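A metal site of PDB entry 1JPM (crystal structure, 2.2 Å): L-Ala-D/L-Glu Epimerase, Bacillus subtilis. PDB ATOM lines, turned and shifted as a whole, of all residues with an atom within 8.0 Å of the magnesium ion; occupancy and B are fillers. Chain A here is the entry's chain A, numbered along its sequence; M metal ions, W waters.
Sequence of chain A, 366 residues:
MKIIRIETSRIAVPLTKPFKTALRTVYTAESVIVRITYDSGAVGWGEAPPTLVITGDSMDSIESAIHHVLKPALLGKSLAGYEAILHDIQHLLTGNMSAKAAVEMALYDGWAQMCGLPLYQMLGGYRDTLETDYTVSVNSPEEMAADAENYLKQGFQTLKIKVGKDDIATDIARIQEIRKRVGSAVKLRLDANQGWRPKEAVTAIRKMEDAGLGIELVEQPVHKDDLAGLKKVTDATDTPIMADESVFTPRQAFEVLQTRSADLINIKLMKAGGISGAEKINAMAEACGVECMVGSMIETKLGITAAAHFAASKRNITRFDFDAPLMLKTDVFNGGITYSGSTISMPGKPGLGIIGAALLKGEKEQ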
ATOM      1  N   ILE A  54       1.803  10.125 -21.646  1.00  0.00           N
ATOM      2  CA  ILE A  54       1.233   9.126 -20.736  1.00  0.00           C
ATOM      3  C   ILE A  54       2.014   8.930 -19.433  1.00  0.00           C
ATOM      4  O   ILE A  54       1.415   8.931 -18.363  1.00  0.00           O
ATOM      5  CB  ILE A  54       1.064   7.757 -21.430  1.00  0.00           C
ATOM      6  CG1 ILE A  54       0.095   7.900 -22.606  1.00  0.00           C
ATOM      7  CG2 ILE A  54       0.544   6.722 -20.427  1.00  0.00           C
ATOM      8  CD1 ILE A  54      -0.109   6.620 -23.399  1.00  0.00           C
ATOM      9  N   LYS A 160     -10.214  -2.637 -32.107  1.00  0.00           N
ATOM     10  CA  LYS A 160     -10.160  -1.573 -31.126  1.00  0.00           C
ATOM     11  C   LYS A 160     -10.359  -0.251 -31.863  1.00  0.00           C
ATOM     12  O   LYS A 160      -9.749  -0.005 -32.907  1.00  0.00           O
ATOM     13  CB  LYS A 160      -8.814  -1.564 -30.403  1.00  0.00           C
ATOM     14  CG  LYS A 160      -8.741  -0.556 -29.270  1.00  0.00           C
ATOM     15  CD  LYS A 160      -7.408  -0.607 -28.517  1.00  0.00           C
ATOM     16  CE  LYS A 160      -6.260  -0.110 -29.380  1.00  0.00           C
ATOM     17  NZ  LYS A 160      -5.040   0.185 -28.562  1.00  0.00           N
ATOM     18  N   LYS A 162     -10.484   3.998 -31.361  1.00  0.00           N
ATOM     19  CA  LYS A 162     -10.233   5.164 -30.544  1.00  0.00           C
ATOM     20  C   LYS A 162     -11.350   6.182 -30.760  1.00  0.00           C
ATOM     21  O   LYS A 162     -11.652   6.552 -31.892  1.00  0.00           O
ATOM     22  CB  LYS A 162      -8.880   5.775 -30.909  1.00  0.00           C
ATOM     23  CG  LYS A 162      -8.656   7.178 -30.387  1.00  0.00           C
ATOM     24  CD  LYS A 162      -8.888   7.278 -28.884  1.00  0.00           C
ATOM     25  CE  LYS A 162      -8.630   8.683 -28.382  1.00  0.00           C
ATOM     26  NZ  LYS A 162      -9.475   9.685 -29.103  1.00  0.00           N
ATOM     27  N   LEU A 190     -13.734   0.023 -27.375  1.00  0.00           N
ATOM     28  CA  LEU A 190     -13.490   1.443 -27.559  1.00  0.00           C
ATOM     29  C   LEU A 190     -12.557   1.966 -26.477  1.00  0.00           C
ATOM     30  O   LEU A 190     -12.530   1.462 -25.342  1.00  0.00           O
ATOM     31  CB  LEU A 190     -14.810   2.236 -27.505  1.00  0.00           C
ATOM     32  CG  LEU A 190     -15.980   1.820 -28.407  1.00  0.00           C
ATOM     33  CD1 LEU A 190     -17.123   2.823 -28.259  1.00  0.00           C
ATOM     34  CD2 LEU A 190     -15.522   1.742 -29.853  1.00  0.00           C
ATOM     35  N   ASP A 191     -11.780   2.982 -26.840  1.00  0.00           N
ATOM     36  CA  ASP A 191     -10.865   3.631 -25.920  1.00  0.00           C
ATOM     37  C   ASP A 191     -11.123   5.132 -26.098  1.00  0.00           C
ATOM     38  O   ASP A 191     -10.781   5.709 -27.132  1.00  0.00           O
ATOM     39  CB  ASP A 191      -9.412   3.308 -26.251  1.00  0.00           C
ATOM     40  CG  ASP A 191      -8.447   3.754 -25.164  1.00  0.00           C
ATOM     41  OD1 ASP A 191      -8.797   4.708 -24.436  1.00  0.00           O
ATOM     42  OD2 ASP A 191      -7.348   3.171 -25.040  1.00  0.00           O
ATOM     43  N   ALA A 192     -11.729   5.763 -25.098  1.00  0.00           N
ATOM     44  CA  ALA A 192     -12.038   7.185 -25.161  1.00  0.00           C
ATOM     45  C   ALA A 192     -10.859   8.061 -24.730  1.00  0.00           C
ATOM     46  O   ALA A 192     -10.931   9.288 -24.816  1.00  0.00           O
ATOM     47  CB  ALA A 192     -13.242   7.481 -24.279  1.00  0.00           C
ATOM     48  N   ASN A 193      -9.774   7.419 -24.301  1.00  0.00           N
ATOM     49  CA  ASN A 193      -8.582   8.144 -23.866  1.00  0.00           C
ATOM     50  C   ASN A 193      -8.901   9.430 -23.090  1.00  0.00           C
ATOM     51  O   ASN A 193      -8.445  10.507 -23.463  1.00  0.00           O
ATOM     52  CB  ASN A 193      -7.686   8.463 -25.067  1.00  0.00           C
ATOM     53  CG  ASN A 193      -6.848   7.256 -25.528  1.00  0.00           C
ATOM     54  OD1 ASN A 193      -5.959   6.784 -24.811  1.00  0.00           O
ATOM     55  ND2 ASN A 193      -7.145   6.742 -26.715  1.00  0.00           N
ATOM     56  N   GLN A 194      -9.680   9.308 -22.018  1.00  0.00           N
ATOM     57  CA  GLN A 194     -10.066  10.419 -21.160  1.00  0.00           C
ATOM     58  C   GLN A 194     -10.706  11.597 -21.894  1.00  0.00           C
ATOM     59  O   GLN A 194     -10.735  12.716 -21.370  1.00  0.00           O
ATOM     60  CB  GLN A 194      -8.829  10.943 -20.401  1.00  0.00           C
ATOM     61  CG  GLN A 194      -7.881   9.878 -19.879  1.00  0.00           C
ATOM     62  CD  GLN A 194      -6.537  10.460 -19.447  1.00  0.00           C
ATOM     63  OE1 GLN A 194      -6.418  11.103 -18.393  1.00  0.00           O
ATOM     64  NE2 GLN A 194      -5.511  10.238 -20.264  1.00  0.00           N
ATOM     65  N   GLU A 219     -12.849   1.874 -22.699  1.00  0.00           N
ATOM     66  CA  GLU A 219     -11.663   2.132 -21.901  1.00  0.00           C
ATOM     67  C   GLU A 219     -11.572   3.608 -21.520  1.00  0.00           C
ATOM     68  O   GLU A 219     -11.839   4.491 -22.337  1.00  0.00           O
ATOM     69  CB  GLU A 219     -10.457   1.727 -22.755  1.00  0.00           C
ATOM     70  CG  GLU A 219      -9.272   1.205 -21.990  1.00  0.00           C
ATOM     71  CD  GLU A 219      -8.153   0.814 -22.923  1.00  0.00           C
ATOM     72  OE1 GLU A 219      -8.401   0.003 -23.845  1.00  0.00           O
ATOM     73  OE2 GLU A 219      -7.026   1.309 -22.746  1.00  0.00           O
ATOM     74  N   GLN A 220     -11.210   3.862 -20.262  1.00  0.00           N
ATOM     75  CA  GLN A 220     -11.010   5.205 -19.691  1.00  0.00           C
ATOM     76  C   GLN A 220     -11.817   6.339 -20.336  1.00  0.00           C
ATOM     77  O   GLN A 220     -11.261   7.202 -21.025  1.00  0.00           O
ATOM     78  CB  GLN A 220      -9.526   5.553 -19.752  1.00  0.00           C
ATOM     79  CG  GLN A 220      -9.084   6.679 -18.846  1.00  0.00           C
ATOM     80  CD  GLN A 220      -9.145   6.301 -17.389  1.00  0.00           C
ATOM     81  OE1 GLN A 220      -8.625   5.254 -16.994  1.00  0.00           O
ATOM     82  NE2 GLN A 220      -9.775   7.137 -16.573  1.00  0.00           N
ATOM     83  N   MET A 242     -13.546   0.002 -18.565  1.00  0.00           N
ATOM     84  CA  MET A 242     -12.197  -0.423 -18.218  1.00  0.00           C
ATOM     85  C   MET A 242     -11.266   0.730 -17.865  1.00  0.00           C
ATOM     86  O   MET A 242     -11.128   1.698 -18.616  1.00  0.00           O
ATOM     87  CB  MET A 242     -11.599  -1.200 -19.394  1.00  0.00           C
ATOM     88  CG  MET A 242     -10.221  -1.777 -19.112  1.00  0.00           C
ATOM     89  SD  MET A 242      -9.532  -2.596 -20.577  1.00  0.00           S
ATOM     90  CE  MET A 242     -10.428  -4.150 -20.569  1.00  0.00           C
ATOM     91  N   ALA A 243     -10.628   0.616 -16.699  1.00  0.00           N
ATOM     92  CA  ALA A 243      -9.694   1.643 -16.280  1.00  0.00           C
ATOM     93  C   ALA A 243      -8.363   1.388 -16.962  1.00  0.00           C
ATOM     94  O   ALA A 243      -7.900   0.255 -17.054  1.00  0.00           O
ATOM     95  CB  ALA A 243      -9.520   1.582 -14.758  1.00  0.00           C
ATOM     96  N   ASP A 244      -7.751   2.454 -17.467  1.00  0.00           N
ATOM     97  CA  ASP A 244      -6.448   2.343 -18.082  1.00  0.00           C
ATOM     98  C   ASP A 244      -5.536   3.358 -17.385  1.00  0.00           C
ATOM     99  O   ASP A 244      -4.870   3.021 -16.405  1.00  0.00           O
ATOM    100  CB  ASP A 244      -6.496   2.633 -19.588  1.00  0.00           C
ATOM    101  CG  ASP A 244      -5.127   2.536 -20.248  1.00  0.00           C
ATOM    102  OD1 ASP A 244      -4.120   2.393 -19.513  1.00  0.00           O
ATOM    103  OD2 ASP A 244      -5.049   2.609 -21.489  1.00  0.00           O
ATOM    104  N   GLU A 245      -5.508   4.596 -17.870  1.00  0.00           N
ATOM    105  CA  GLU A 245      -4.656   5.607 -17.266  1.00  0.00           C
ATOM    106  C   GLU A 245      -4.953   5.899 -15.787  1.00  0.00           C
ATOM    107  O   GLU A 245      -4.118   6.499 -15.108  1.00  0.00           O
ATOM    108  CB  GLU A 245      -4.702   6.901 -18.082  1.00  0.00           C
ATOM    109  CG  GLU A 245      -3.964   6.846 -19.423  1.00  0.00           C
ATOM    110  CD  GLU A 245      -4.750   6.128 -20.521  1.00  0.00           C
ATOM    111  OE1 GLU A 245      -5.936   5.817 -20.308  1.00  0.00           O
ATOM    112  OE2 GLU A 245      -4.177   5.901 -21.599  1.00  0.00           O
ATOM    113  N   ASN A 266      -6.983  -2.287 -17.392  1.00  0.00           N
ATOM    114  CA  ASN A 266      -6.035  -2.538 -18.465  1.00  0.00           C
ATOM    115  C   ASN A 266      -4.637  -2.343 -17.900  1.00  0.00           C
ATOM    116  O   ASN A 266      -4.271  -1.243 -17.467  1.00  0.00           O
ATOM    117  CB  ASN A 266      -6.259  -1.566 -19.632  1.00  0.00           C
ATOM    118  CG  ASN A 266      -5.394  -1.899 -20.843  1.00  0.00           C
ATOM    119  OD1 ASN A 266      -5.319  -1.137 -21.808  1.00  0.00           O
ATOM    120  ND2 ASN A 266      -4.745  -3.059 -20.797  1.00  0.00           N
ATOM    121  N   LYS A 268      -0.466  -2.332 -18.210  1.00  0.00           N
ATOM    122  CA  LYS A 268       0.611  -2.105 -19.177  1.00  0.00           C
ATOM    123  C   LYS A 268       1.926  -2.074 -18.389  1.00  0.00           C
ATOM    124  O   LYS A 268       2.036  -1.354 -17.378  1.00  0.00           O
ATOM    125  CB  LYS A 268       0.421  -0.782 -19.919  1.00  0.00           C
ATOM    126  CG  LYS A 268      -0.775  -0.730 -20.865  1.00  0.00           C
ATOM    127  CD  LYS A 268      -0.753   0.574 -21.667  1.00  0.00           C
ATOM    128  CE  LYS A 268      -2.061   0.800 -22.415  1.00  0.00           C
ATOM    129  NZ  LYS A 268      -2.111   2.149 -23.047  1.00  0.00           N
ATOM    130  N   LYS A 271       3.458   1.309 -17.463  1.00  0.00           N
ATOM    131  CA  LYS A 271       2.782   2.028 -16.396  1.00  0.00           C
ATOM    132  C   LYS A 271       3.106   1.447 -15.031  1.00  0.00           C
ATOM    133  O   LYS A 271       3.330   2.186 -14.082  1.00  0.00           O
ATOM    134  CB  LYS A 271       1.258   1.988 -16.584  1.00  0.00           C
ATOM    135  CG  LYS A 271       0.735   2.652 -17.861  1.00  0.00           C
ATOM    136  CD  LYS A 271      -0.807   2.654 -17.889  1.00  0.00           C
ATOM    137  CE  LYS A 271      -1.388   1.260 -17.614  1.00  0.00           C
ATOM    138  NZ  LYS A 271      -2.873   1.264 -17.441  1.00  0.00           N
ATOM    139  N   MET A 293      -6.975  -6.816 -18.719  1.00  0.00           N
ATOM    140  CA  MET A 293      -6.551  -6.904 -20.107  1.00  0.00           C
ATOM    141  C   MET A 293      -5.127  -6.421 -20.044  1.00  0.00           C
ATOM    142  O   MET A 293      -4.751  -5.696 -19.118  1.00  0.00           O
ATOM    143  CB  MET A 293      -7.371  -5.963 -21.000  1.00  0.00           C
ATOM    144  CG  MET A 293      -6.910  -5.931 -22.466  1.00  0.00           C
ATOM    145  SD  MET A 293      -8.004  -4.968 -23.559  1.00  0.00           S
ATOM    146  CE  MET A 293      -7.184  -3.353 -23.566  1.00  0.00           C
ATOM    147  N   GLY A 295      -2.241  -4.471 -22.339  1.00  0.00           N
ATOM    148  CA  GLY A 295      -1.978  -3.747 -23.572  1.00  0.00           C
ATOM    149  C   GLY A 295      -0.527  -3.339 -23.586  1.00  0.00           C
ATOM    150  O   GLY A 295       0.316  -4.018 -22.999  1.00  0.00           O
ATOM    151  N   SER A 296      -0.224  -2.222 -24.250  1.00  0.00           N
ATOM    152  CA  SER A 296       1.142  -1.738 -24.330  1.00  0.00           C
ATOM    153  C   SER A 296       1.189  -0.359 -24.992  1.00  0.00           C
ATOM    154  O   SER A 296       0.168   0.180 -25.409  1.00  0.00           O
ATOM    155  CB  SER A 296       1.990  -2.680 -25.172  1.00  0.00           C
ATOM    156  OG  SER A 296       1.708  -2.480 -26.552  1.00  0.00           O
ATOM    157  N   MET A 297       2.385   0.195 -25.071  1.00  0.00           N
ATOM    158  CA  MET A 297       2.593   1.472 -25.735  1.00  0.00           C
ATOM    159  C   MET A 297       3.075   1.097 -27.139  1.00  0.00           C
ATOM    160  O   MET A 297       2.968  -0.060 -27.546  1.00  0.00           O
ATOM    161  CB  MET A 297       3.668   2.288 -24.991  1.00  0.00           C
ATOM    162  CG  MET A 297       3.388   2.512 -23.512  1.00  0.00           C
ATOM    163  SD  MET A 297       1.765   3.286 -23.228  1.00  0.00           S
ATOM    164  CE  MET A 297       1.798   3.444 -21.400  1.00  0.00           C
ATOM    165  N   ASP A 321      -4.311  -6.790 -26.002  1.00  0.00           N
ATOM    166  CA  ASP A 321      -4.222  -5.735 -26.987  1.00  0.00           C
ATOM    167  C   ASP A 321      -2.768  -5.591 -27.415  1.00  0.00           C
ATOM    168  O   ASP A 321      -2.063  -4.682 -26.976  1.00  0.00           O
ATOM    169  CB  ASP A 321      -4.731  -4.434 -26.355  1.00  0.00           C
ATOM    170  CG  ASP A 321      -4.749  -3.279 -27.311  1.00  0.00           C
ATOM    171  OD1 ASP A 321      -4.779  -2.124 -26.840  1.00  0.00           O
ATOM    172  OD2 ASP A 321      -4.726  -3.514 -28.542  1.00  0.00           O
HETATM  173 MG    MG M   1      -6.051   2.947 -23.343  1.00  0.00          MG
HETATM  174  O   HOH W   1      -4.654   1.578 -24.418  1.00  0.00           O
HETATM  175  O   HOH W   2      -7.421   4.441 -22.269  1.00  0.00           O
HETATM  176  O   HOH W   3      -4.759   4.664 -23.699  1.00  0.00           O
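Water W2 bridges the side-chain carboxylate (OD1) of Asp 191 and the side-chain carboxylate (OE1) of Glu 245. Water W3 lies within hydrogen-bond range of the side-chain carboxylate (OE2) of Glu 245 (2.5 Å) and the side-chain amide oxygen (OD1) of Asn 193 (2.7 Å).
The side-chain carboxylate of Glu 219 lies close to the side-chain amide oxygen of Asn 266 (3.1 Å). The backbone NH (N) of Ala 192 lies within hydrogen-bond range of the backbone carbonyl oxygen (O) of Glu 219, 3.0 Å away. The backbone NH of Glu 219 is in hydrogen-bond range of the backbone carbonyl oxygen of Leu 190, 2.7 Å away. The side-chain carboxylate (OD2) of Asp 244 lies close to the side-chain amino group (NZ) of Lys 268. N of Asp 244 is in hydrogen-bond range of OE1 of Gln 220 (3.0 Å). OD1 of Asp 244 lies within salt-bridge range of NZ of Lys 271 (2.7 Å). The side-chain carboxylate (OD1) of Asp 191 is in hydrogen-bond range of the backbone NH (N) of Asn 193. The backbone NH of Glu 245 lies within hydrogen-bond range of the side-chain amide oxygen of Gln 220 (3.3 Å).
OE2 of Glu 219 binds the magnesium ion (2.0 Å). The side-chain carboxylate (OD2) of Asp 244 is bound to the magnesium ion (2.1 Å). The magnesium ion is bound by the side-chain carboxylate (OD2) of Asp 191, at 2.1 Å. The magnesium ion is bound by water W3, at 2.2 Å. The magnesium ion is bound by water W1 (2.2 Å). Water W2 binds the magnesium ion (2.3 Å).
Glu 245 touches the magnesium ion. Within 4 Å of the magnesium ion: Asp 191, Glu 219, Asp 244 and Glu 245.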
